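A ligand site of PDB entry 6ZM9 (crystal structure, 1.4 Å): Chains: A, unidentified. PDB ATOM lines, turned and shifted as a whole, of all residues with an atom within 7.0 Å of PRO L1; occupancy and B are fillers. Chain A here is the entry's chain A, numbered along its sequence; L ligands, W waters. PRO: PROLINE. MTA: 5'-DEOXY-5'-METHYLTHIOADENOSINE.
The side-chain amide oxygen (OE1) of Gln 104 sits at hydrogen-bond distance from a nitrogen (N) of PRO L1 (2.7 Å).
The side-chain carboxylate (OE1) of Glu 69 is in salt-bridge range of a nitrogen (N) of PRO L1 (2.6 Å).
The backbone NH (N) of Gly 22 is in hydrogen-bond range of an oxygen (O) of PRO L1.
An oxygen (O2') of MTA L2 is in hydrogen-bond range of the side-chain hydroxyl (OG) of Ser 71 (2.8 Å).
The side-chain carboxylate of Glu 69 lies within hydrogen-bond range of an oxygen (O3') of MTA L2, 2.6 Å away.
An oxygen (OXT) of PRO L1 lies within hydrogen-bond range of the backbone NH (N) of Glu 105 (2.9 Å).
The backbone carbonyl oxygen of Asn 20 sits at hydrogen-bond distance from a nitrogen (N) of PRO L1, at 3.2 Å.
Val 21 touches PRO L1.
Tyr 58 touches PRO L1 (CD2 to CG, 3.1 Å).
Hydrophobic or aromatic side chains within 4 Å of PRO L1: Tyr 58.
Within 4 Å of PRO L1: Asn 20, Val 21, Gly 22, Tyr 58, Glu 69, Gln 104 and Glu 105.
The nearest printed residue that does not touch PRO L1 is Gly 18 (4.1 Å).
O of Tyr 58 is in hydrogen-bond range of N of Val 67 (2.8 Å).
The backbone NH of Asn 20 sits at hydrogen-bond distance from the side-chain carboxylate of Glu 69, at 3.1 Å.
NE2 of Gln 104 sits at hydrogen-bond distance from O of Asn 20 (2.8 Å).
The side-chain hydroxyl (OH) of Tyr 58 is in hydrogen-bond range of the side-chain carboxylate (OE1) of Glu 105 (2.4 Å).
OE1 of Glu 69 lies within hydrogen-bond range of N of Leu 19, at 3.5 Å.
The backbone carbonyl oxygen of Gly 22 sits at hydrogen-bond distance from the side-chain amide nitrogen of Asn 20 (3.1 Å).
O of Gly 18 sits close to OE1 of Gln 104, 3.4 Å away.
The backbone carbonyl oxygen of Phe 102 lies within hydrogen-bond range of the side-chain amide nitrogen of Gln 104 (2.8 Å).
Water W2 bridges O of Lys 103 (2.6 Å) and O of PRO L1 (2.6 Å).
Water W1 lies within hydrogen-bond range of an oxygen (O) of PRO L1 (2.8 Å) and the side-chain carboxylate (OE2) of Glu 60 (3.4 Å).
Water W3 lies within hydrogen-bond range of N of Ser 106 (2.8 Å), OXT of PRO L1 (3.0 Å), N of Glu 105 (3.4 Å) and S5' of MTA L2 (3.8 Å).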
ATOM      1  N   VAL A  17     -21.665   8.435  -8.815  1.00  0.00           N
ATOM      2  CA  VAL A  17     -21.514   9.738  -8.158  1.00  0.00           C
ATOM      3  C   VAL A  17     -22.895  10.278  -7.831  1.00  0.00           C
ATOM      4  O   VAL A  17     -23.692  10.500  -8.754  1.00  0.00           O
ATOM      5  CB  VAL A  17     -20.781  10.769  -9.045  1.00  0.00           C
ATOM      6  CG1 VAL A  17     -20.487  12.038  -8.232  1.00  0.00           C
ATOM      7  CG2 VAL A  17     -19.505  10.220  -9.655  1.00  0.00           C
ATOM      8  N   GLY A  18     -23.165  10.544  -6.557  1.00  0.00           N
ATOM      9  CA  GLY A  18     -24.407  11.164  -6.173  1.00  0.00           C
ATOM     10  C   GLY A  18     -24.408  12.677  -6.346  1.00  0.00           C
ATOM     11  O   GLY A  18     -23.371  13.340  -6.473  1.00  0.00           O
ATOM     12  N   LEU A  19     -25.627  13.237  -6.361  1.00  0.00           N
ATOM     13  CA  LEU A  19     -25.846  14.657  -6.652  1.00  0.00           C
ATOM     14  C   LEU A  19     -26.468  15.398  -5.479  1.00  0.00           C
ATOM     15  O   LEU A  19     -26.662  16.618  -5.566  1.00  0.00           O
ATOM     16  CB  LEU A  19     -26.706  14.819  -7.913  1.00  0.00           C
ATOM     17  CG  LEU A  19     -26.082  14.184  -9.163  1.00  0.00           C
ATOM     18  CD1 LEU A  19     -27.065  14.265 -10.303  1.00  0.00           C
ATOM     19  CD2 LEU A  19     -24.768  14.824  -9.540  1.00  0.00           C
ATOM     20  N   ASN A  20     -26.773  14.712  -4.387  1.00  0.00           N
ATOM     21  CA  ASN A  20     -27.132  15.360  -3.140  1.00  0.00           C
ATOM     22  C   ASN A  20     -25.864  15.632  -2.343  1.00  0.00           C
ATOM     23  O   ASN A  20     -24.883  14.890  -2.430  1.00  0.00           O
ATOM     24  CB  ASN A  20     -27.948  14.417  -2.254  1.00  0.00           C
ATOM     25  CG  ASN A  20     -29.448  14.591  -2.390  1.00  0.00           C
ATOM     26  OD1 ASN A  20     -29.967  14.929  -3.442  1.00  0.00           O
ATOM     27  ND2 ASN A  20     -30.152  14.284  -1.301  1.00  0.00           N
ATOM     28  N   VAL A  21     -25.926  16.661  -1.501  1.00  0.00           N
ATOM     29  CA  VAL A  21     -24.983  16.851  -0.402  1.00  0.00           C
ATOM     30  C   VAL A  21     -25.806  16.609   0.858  1.00  0.00           C
ATOM     31  O   VAL A  21     -26.705  17.406   1.183  1.00  0.00           O
ATOM     32  CB  VAL A  21     -24.337  18.240  -0.426  1.00  0.00           C
ATOM     33  CG1 VAL A  21     -23.431  18.378   0.763  1.00  0.00           C
ATOM     34  CG2 VAL A  21     -23.571  18.441  -1.745  1.00  0.00           C
ATOM     35  N   GLY A  22     -25.586  15.466   1.501  1.00  0.00           N
ATOM     36  CA  GLY A  22     -26.479  15.066   2.573  1.00  0.00           C
ATOM     37  C   GLY A  22     -27.890  14.913   2.055  1.00  0.00           C
ATOM     38  O   GLY A  22     -28.132  14.223   1.052  1.00  0.00           O
ATOM     39  N   ASP A  23     -28.853  15.544   2.722  1.00  0.00           N
ATOM     40  CA  ASP A  23     -30.241  15.428   2.285  1.00  0.00           C
ATOM     41  C   ASP A  23     -30.657  16.500   1.270  1.00  0.00           C
ATOM     42  O   ASP A  23     -31.831  16.559   0.907  1.00  0.00           O
ATOM     43  CB  ASP A  23     -31.202  15.419   3.487  1.00  0.00           C
ATOM     44  CG  ASP A  23     -31.162  16.712   4.287  1.00  0.00           C
ATOM     45  OD1 ASP A  23     -30.668  17.729   3.771  1.00  0.00           O
ATOM     46  OD2 ASP A  23     -31.615  16.680   5.453  1.00  0.00           O
ATOM     47  N   VAL A  57     -30.070   5.254  -3.921  1.00  0.00           N
ATOM     48  CA  VAL A  57     -30.355   5.104  -2.507  1.00  0.00           C
ATOM     49  C   VAL A  57     -29.037   4.762  -1.815  1.00  0.00           C
ATOM     50  O   VAL A  57     -28.335   3.844  -2.257  1.00  0.00           O
ATOM     51  CB  VAL A  57     -31.400   4.005  -2.277  1.00  0.00           C
ATOM     52  CG1 VAL A  57     -31.623   3.725  -0.804  1.00  0.00           C
ATOM     53  CG2 VAL A  57     -32.712   4.381  -2.957  1.00  0.00           C
ATOM     54  N   TYR A  58     -28.717   5.493  -0.749  1.00  0.00           N
ATOM     55  CA  TYR A  58     -27.472   5.344  -0.025  1.00  0.00           C
ATOM     56  C   TYR A  58     -27.703   5.537   1.467  1.00  0.00           C
ATOM     57  O   TYR A  58     -28.399   6.458   1.881  1.00  0.00           O
ATOM     58  CB  TYR A  58     -26.488   6.395  -0.497  1.00  0.00           C
ATOM     59  CG  TYR A  58     -25.185   6.481   0.253  1.00  0.00           C
ATOM     60  CD1 TYR A  58     -24.168   5.569   0.014  1.00  0.00           C
ATOM     61  CD2 TYR A  58     -24.958   7.467   1.186  1.00  0.00           C
ATOM     62  CE1 TYR A  58     -22.936   5.653   0.670  1.00  0.00           C
ATOM     63  CE2 TYR A  58     -23.738   7.571   1.849  1.00  0.00           C
ATOM     64  CZ  TYR A  58     -22.739   6.638   1.597  1.00  0.00           C
ATOM     65  OH  TYR A  58     -21.514   6.722   2.236  1.00  0.00           O
ATOM     66  N   THR A  59     -27.075   4.678   2.269  1.00  0.00           N
ATOM     67  CA  THR A  59     -27.122   4.798   3.720  1.00  0.00           C
ATOM     68  C   THR A  59     -25.882   5.544   4.184  1.00  0.00           C
ATOM     69  O   THR A  59     -24.755   5.060   3.992  1.00  0.00           O
ATOM     70  CB  THR A  59     -27.197   3.433   4.391  1.00  0.00           C
ATOM     71  OG1 THR A  59     -28.361   2.746   3.947  1.00  0.00           O
ATOM     72  CG2 THR A  59     -27.259   3.597   5.907  1.00  0.00           C
ATOM     73  N   GLU A  60     -26.071   6.723   4.775  1.00  0.00           N
ATOM     74  CA  GLU A  60     -24.941   7.489   5.277  1.00  0.00           C
ATOM     75  C   GLU A  60     -24.236   6.714   6.385  1.00  0.00           C
ATOM     76  O   GLU A  60     -24.870   6.210   7.312  1.00  0.00           O
ATOM     77  CB  GLU A  60     -25.395   8.827   5.844  1.00  0.00           C
ATOM     78  CG  GLU A  60     -25.987   9.750   4.808  1.00  0.00           C
ATOM     79  CD  GLU A  60     -26.278  11.125   5.368  1.00  0.00           C
ATOM     80  OE1 GLU A  60     -26.011  11.352   6.573  1.00  0.00           O
ATOM     81  OE2 GLU A  60     -26.759  11.967   4.601  1.00  0.00           O
ATOM     82  N   VAL A  67     -30.622   8.135   2.308  1.00  0.00           N
ATOM     83  CA  VAL A  67     -30.826   9.212   1.351  1.00  0.00           C
ATOM     84  C   VAL A  67     -31.270   8.632   0.020  1.00  0.00           C
ATOM     85  O   VAL A  67     -30.702   7.647  -0.462  1.00  0.00           O
ATOM     86  CB  VAL A  67     -29.507   9.992   1.176  1.00  0.00           C
ATOM     87  CG1 VAL A  67     -29.638  11.075   0.111  1.00  0.00           C
ATOM     88  CG2 VAL A  67     -29.050  10.582   2.489  1.00  0.00           C
ATOM     89  N   GLU A  69     -31.601  10.127  -3.865  1.00  0.00           N
ATOM     90  CA  GLU A  69     -31.040  11.263  -4.575  1.00  0.00           C
ATOM     91  C   GLU A  69     -31.030  10.967  -6.070  1.00  0.00           C
ATOM     92  O   GLU A  69     -31.220   9.844  -6.516  1.00  0.00           O
ATOM     93  CB  GLU A  69     -29.590  11.529  -4.119  1.00  0.00           C
ATOM     94  CG  GLU A  69     -28.649  10.328  -4.342  1.00  0.00           C
ATOM     95  CD  GLU A  69     -27.201  10.569  -3.918  1.00  0.00           C
ATOM     96  OE1 GLU A  69     -26.849  11.711  -3.517  1.00  0.00           O
ATOM     97  OE2 GLU A  69     -26.410   9.612  -3.997  1.00  0.00           O
ATOM     98  N   ASN A  70     -30.791  12.015  -6.846  1.00  0.00           N
ATOM     99  CA  ASN A  70     -30.330  11.815  -8.212  1.00  0.00           C
ATOM    100  C   ASN A  70     -28.855  11.442  -8.179  1.00  0.00           C
ATOM    101  O   ASN A  70     -28.108  11.911  -7.311  1.00  0.00           O
ATOM    102  CB  ASN A  70     -30.497  13.089  -9.035  1.00  0.00           C
ATOM    103  CG  ASN A  70     -31.935  13.464  -9.249  1.00  0.00           C
ATOM    104  OD1 ASN A  70     -32.837  12.618  -9.256  1.00  0.00           O
ATOM    105  ND2 ASN A  70     -32.165  14.749  -9.468  1.00  0.00           N
ATOM    106  N   SER A  71     -28.434  10.593  -9.106  1.00  0.00           N
ATOM    107  CA  SER A  71     -27.035  10.220  -9.197  1.00  0.00           C
ATOM    108  C   SER A  71     -26.667   9.973 -10.652  1.00  0.00           C
ATOM    109  O   SER A  71     -27.515  10.027 -11.550  1.00  0.00           O
ATOM    110  CB  SER A  71     -26.699   9.013  -8.312  1.00  0.00           C
ATOM    111  OG  SER A  71     -27.390   7.873  -8.752  1.00  0.00           O
ATOM    112  N   PHE A 102     -17.674  17.140  -5.840  1.00  0.00           N
ATOM    113  CA  PHE A 102     -19.102  17.098  -5.547  1.00  0.00           C
ATOM    114  C   PHE A 102     -19.382  16.906  -4.056  1.00  0.00           C
ATOM    115  O   PHE A 102     -20.536  16.699  -3.679  1.00  0.00           O
ATOM    116  CB  PHE A 102     -19.787  16.105  -6.486  1.00  0.00           C
ATOM    117  CG  PHE A 102     -19.744  16.571  -7.906  1.00  0.00           C
ATOM    118  CD1 PHE A 102     -20.540  17.618  -8.319  1.00  0.00           C
ATOM    119  CD2 PHE A 102     -18.801  16.063  -8.790  1.00  0.00           C
ATOM    120  CE1 PHE A 102     -20.454  18.111  -9.604  1.00  0.00           C
ATOM    121  CE2 PHE A 102     -18.712  16.565 -10.095  1.00  0.00           C
ATOM    122  CZ  PHE A 102     -19.540  17.588 -10.495  1.00  0.00           C
ATOM    123  N   LYS A 103     -18.365  17.070  -3.212  1.00  0.00           N
ATOM    124  CA  LYS A 103     -18.543  17.120  -1.759  1.00  0.00           C
ATOM    125  C   LYS A 103     -19.213  15.853  -1.243  1.00  0.00           C
ATOM    126  O   LYS A 103     -20.045  15.909  -0.334  1.00  0.00           O
ATOM    127  CB  LYS A 103     -19.312  18.370  -1.337  1.00  0.00           C
ATOM    128  CG  LYS A 103     -18.636  19.664  -1.740  1.00  0.00           C
ATOM    129  CD  LYS A 103     -19.438  20.849  -1.244  1.00  0.00           C
ATOM    130  CE  LYS A 103     -18.810  22.177  -1.568  1.00  0.00           C
ATOM    131  NZ  LYS A 103     -19.679  23.271  -1.035  1.00  0.00           N
ATOM    132  N   GLN A 104     -18.835  14.717  -1.813  1.00  0.00           N
ATOM    133  CA  GLN A 104     -19.508  13.454  -1.529  1.00  0.00           C
ATOM    134  C   GLN A 104     -18.859  12.668  -0.397  1.00  0.00           C
ATOM    135  O   GLN A 104     -17.639  12.670  -0.222  1.00  0.00           O
ATOM    136  CB  GLN A 104     -19.519  12.576  -2.785  1.00  0.00           C
ATOM    137  CG  GLN A 104     -20.295  13.179  -3.923  1.00  0.00           C
ATOM    138  CD  GLN A 104     -21.755  13.253  -3.590  1.00  0.00           C
ATOM    139  OE1 GLN A 104     -22.417  12.229  -3.441  1.00  0.00           O
ATOM    140  NE2 GLN A 104     -22.280  14.467  -3.455  1.00  0.00           N
ATOM    141  N   GLU A 105     -19.700  11.922   0.327  1.00  0.00           N
ATOM    142  CA  GLU A 105     -19.200  11.024   1.361  1.00  0.00           C
ATOM    143  C   GLU A 105     -18.503   9.823   0.733  1.00  0.00           C
ATOM    144  O   GLU A 105     -17.471   9.361   1.248  1.00  0.00           O
ATOM    145  CB  GLU A 105     -20.313  10.540   2.279  1.00  0.00           C
ATOM    146  CG  GLU A 105     -19.734   9.761   3.455  1.00  0.00           C
ATOM    147  CD  GLU A 105     -20.768   9.195   4.396  1.00  0.00           C
ATOM    148  OE1 GLU A 105     -21.654   8.429   3.951  1.00  0.00           O
ATOM    149  OE2 GLU A 105     -20.676   9.514   5.588  1.00  0.00           O
ATOM    150  N   SER A 106     -19.048   9.297  -0.360  1.00  0.00           N
ATOM    151  CA  SER A 106     -18.564   8.071  -0.990  1.00  0.00           C
ATOM    152  C   SER A 106     -18.799   8.133  -2.488  1.00  0.00           C
ATOM    153  O   SER A 106     -19.881   8.563  -2.907  1.00  0.00           O
ATOM    154  CB  SER A 106     -19.396   6.893  -0.441  1.00  0.00           C
ATOM    155  OG  SER A 106     -18.952   5.639  -0.922  1.00  0.00           O
ATOM    156  N   VAL A 107     -17.838   7.646  -3.265  1.00  0.00           N
ATOM    157  CA  VAL A 107     -17.965   7.395  -4.697  1.00  0.00           C
ATOM    158  C   VAL A 107     -17.578   5.933  -4.919  1.00  0.00           C
ATOM    159  O   VAL A 107     -16.562   5.482  -4.378  1.00  0.00           O
ATOM    160  CB  VAL A 107     -17.077   8.343  -5.531  1.00  0.00           C
ATOM    161  CG1 VAL A 107     -16.912   7.886  -6.960  1.00  0.00           C
ATOM    162  CG2 VAL A 107     -17.666   9.756  -5.514  1.00  0.00           C
ATOM    163  N   TRP A 127     -13.482  12.908   6.502  1.00  0.00           N
ATOM    164  CA  TRP A 127     -13.930  13.965   7.378  1.00  0.00           C
ATOM    165  C   TRP A 127     -13.730  13.599   8.848  1.00  0.00           C
ATOM    166  O   TRP A 127     -14.157  12.526   9.294  1.00  0.00           O
ATOM    167  CB  TRP A 127     -15.417  14.221   7.121  1.00  0.00           C
ATOM    168  CG  TRP A 127     -15.758  14.591   5.695  1.00  0.00           C
ATOM    169  CD1 TRP A 127     -14.985  15.290   4.808  1.00  0.00           C
ATOM    170  CD2 TRP A 127     -16.969  14.283   5.023  1.00  0.00           C
ATOM    171  NE1 TRP A 127     -15.651  15.434   3.606  1.00  0.00           N
ATOM    172  CE2 TRP A 127     -16.882  14.826   3.721  1.00  0.00           C
ATOM    173  CE3 TRP A 127     -18.136  13.608   5.384  1.00  0.00           C
ATOM    174  CZ2 TRP A 127     -17.903  14.711   2.794  1.00  0.00           C
ATOM    175  CZ3 TRP A 127     -19.155  13.486   4.449  1.00  0.00           C
ATOM    176  CH2 TRP A 127     -19.023  14.023   3.178  1.00  0.00           C
HETATM  177  N   PRO L   1     -24.658  11.717  -2.051  1.00  0.00           N
HETATM  178  CA  PRO L   1     -24.896  12.095  -0.652  1.00  0.00           C
HETATM  179  C   PRO L   1     -23.657  12.630   0.046  1.00  0.00           C
HETATM  180  O   PRO L   1     -23.761  13.437   0.975  1.00  0.00           O
HETATM  181  CB  PRO L   1     -25.293  10.760  -0.015  1.00  0.00           C
HETATM  182  CG  PRO L   1     -24.667   9.709  -0.962  1.00  0.00           C
HETATM  183  CD  PRO L   1     -24.069  10.381  -2.134  1.00  0.00           C
HETATM  184  OXT PRO L   1     -22.543  12.243  -0.299  1.00  0.00           O
HETATM  185  CS  MTA L   2     -22.015   5.887  -3.302  1.00  0.00           C
HETATM  186  S5' MTA L   2     -23.460   6.883  -3.127  1.00  0.00           S
HETATM  187  C5' MTA L   2     -23.673   7.465  -4.812  1.00  0.00           C
HETATM  188  C4' MTA L   2     -24.569   6.614  -5.695  1.00  0.00           C
HETATM  189  O4' MTA L   2     -24.020   5.283  -5.777  1.00  0.00           O
HETATM  190  C2' MTA L   2     -26.410   5.152  -6.006  1.00  0.00           C
HETATM  191  O2' MTA L   2     -26.788   5.553  -7.306  1.00  0.00           O
HETATM  192  C3' MTA L   2     -26.016   6.414  -5.231  1.00  0.00           C
HETATM  193  O3' MTA L   2     -26.851   7.527  -5.509  1.00  0.00           O
HETATM  194  C1' MTA L   2     -25.082   4.380  -6.039  1.00  0.00           C
HETATM  195  N9  MTA L   2     -25.025   3.301  -5.061  1.00  0.00           N
HETATM  196  C8  MTA L   2     -24.677   3.358  -3.732  1.00  0.00           C
HETATM  197  N7  MTA L   2     -24.620   2.197  -3.139  1.00  0.00           N
HETATM  198  C5  MTA L   2     -24.970   1.296  -4.133  1.00  0.00           C
HETATM  199  C6  MTA L   2     -25.021  -0.110  -4.170  1.00  0.00           C
HETATM  200  N6  MTA L   2     -24.718  -0.904  -3.138  1.00  0.00           N
HETATM  201  N1  MTA L   2     -25.362  -0.689  -5.357  1.00  0.00           N
HETATM  202  C2  MTA L   2     -25.609   0.095  -6.408  1.00  0.00           C
HETATM  203  N3  MTA L   2     -25.569   1.419  -6.503  1.00  0.00           N
HETATM  204  C4  MTA L   2     -25.237   1.970  -5.320  1.00  0.00           C
HETATM  205  O   HOH W   1     -23.585  12.207   3.434  1.00  0.00           O
HETATM  206  O   HOH W   2     -21.791  15.138   1.472  1.00  0.00           O
HETATM  207  O   HOH W   3     -21.754   9.470  -0.936  1.00  0.00           O
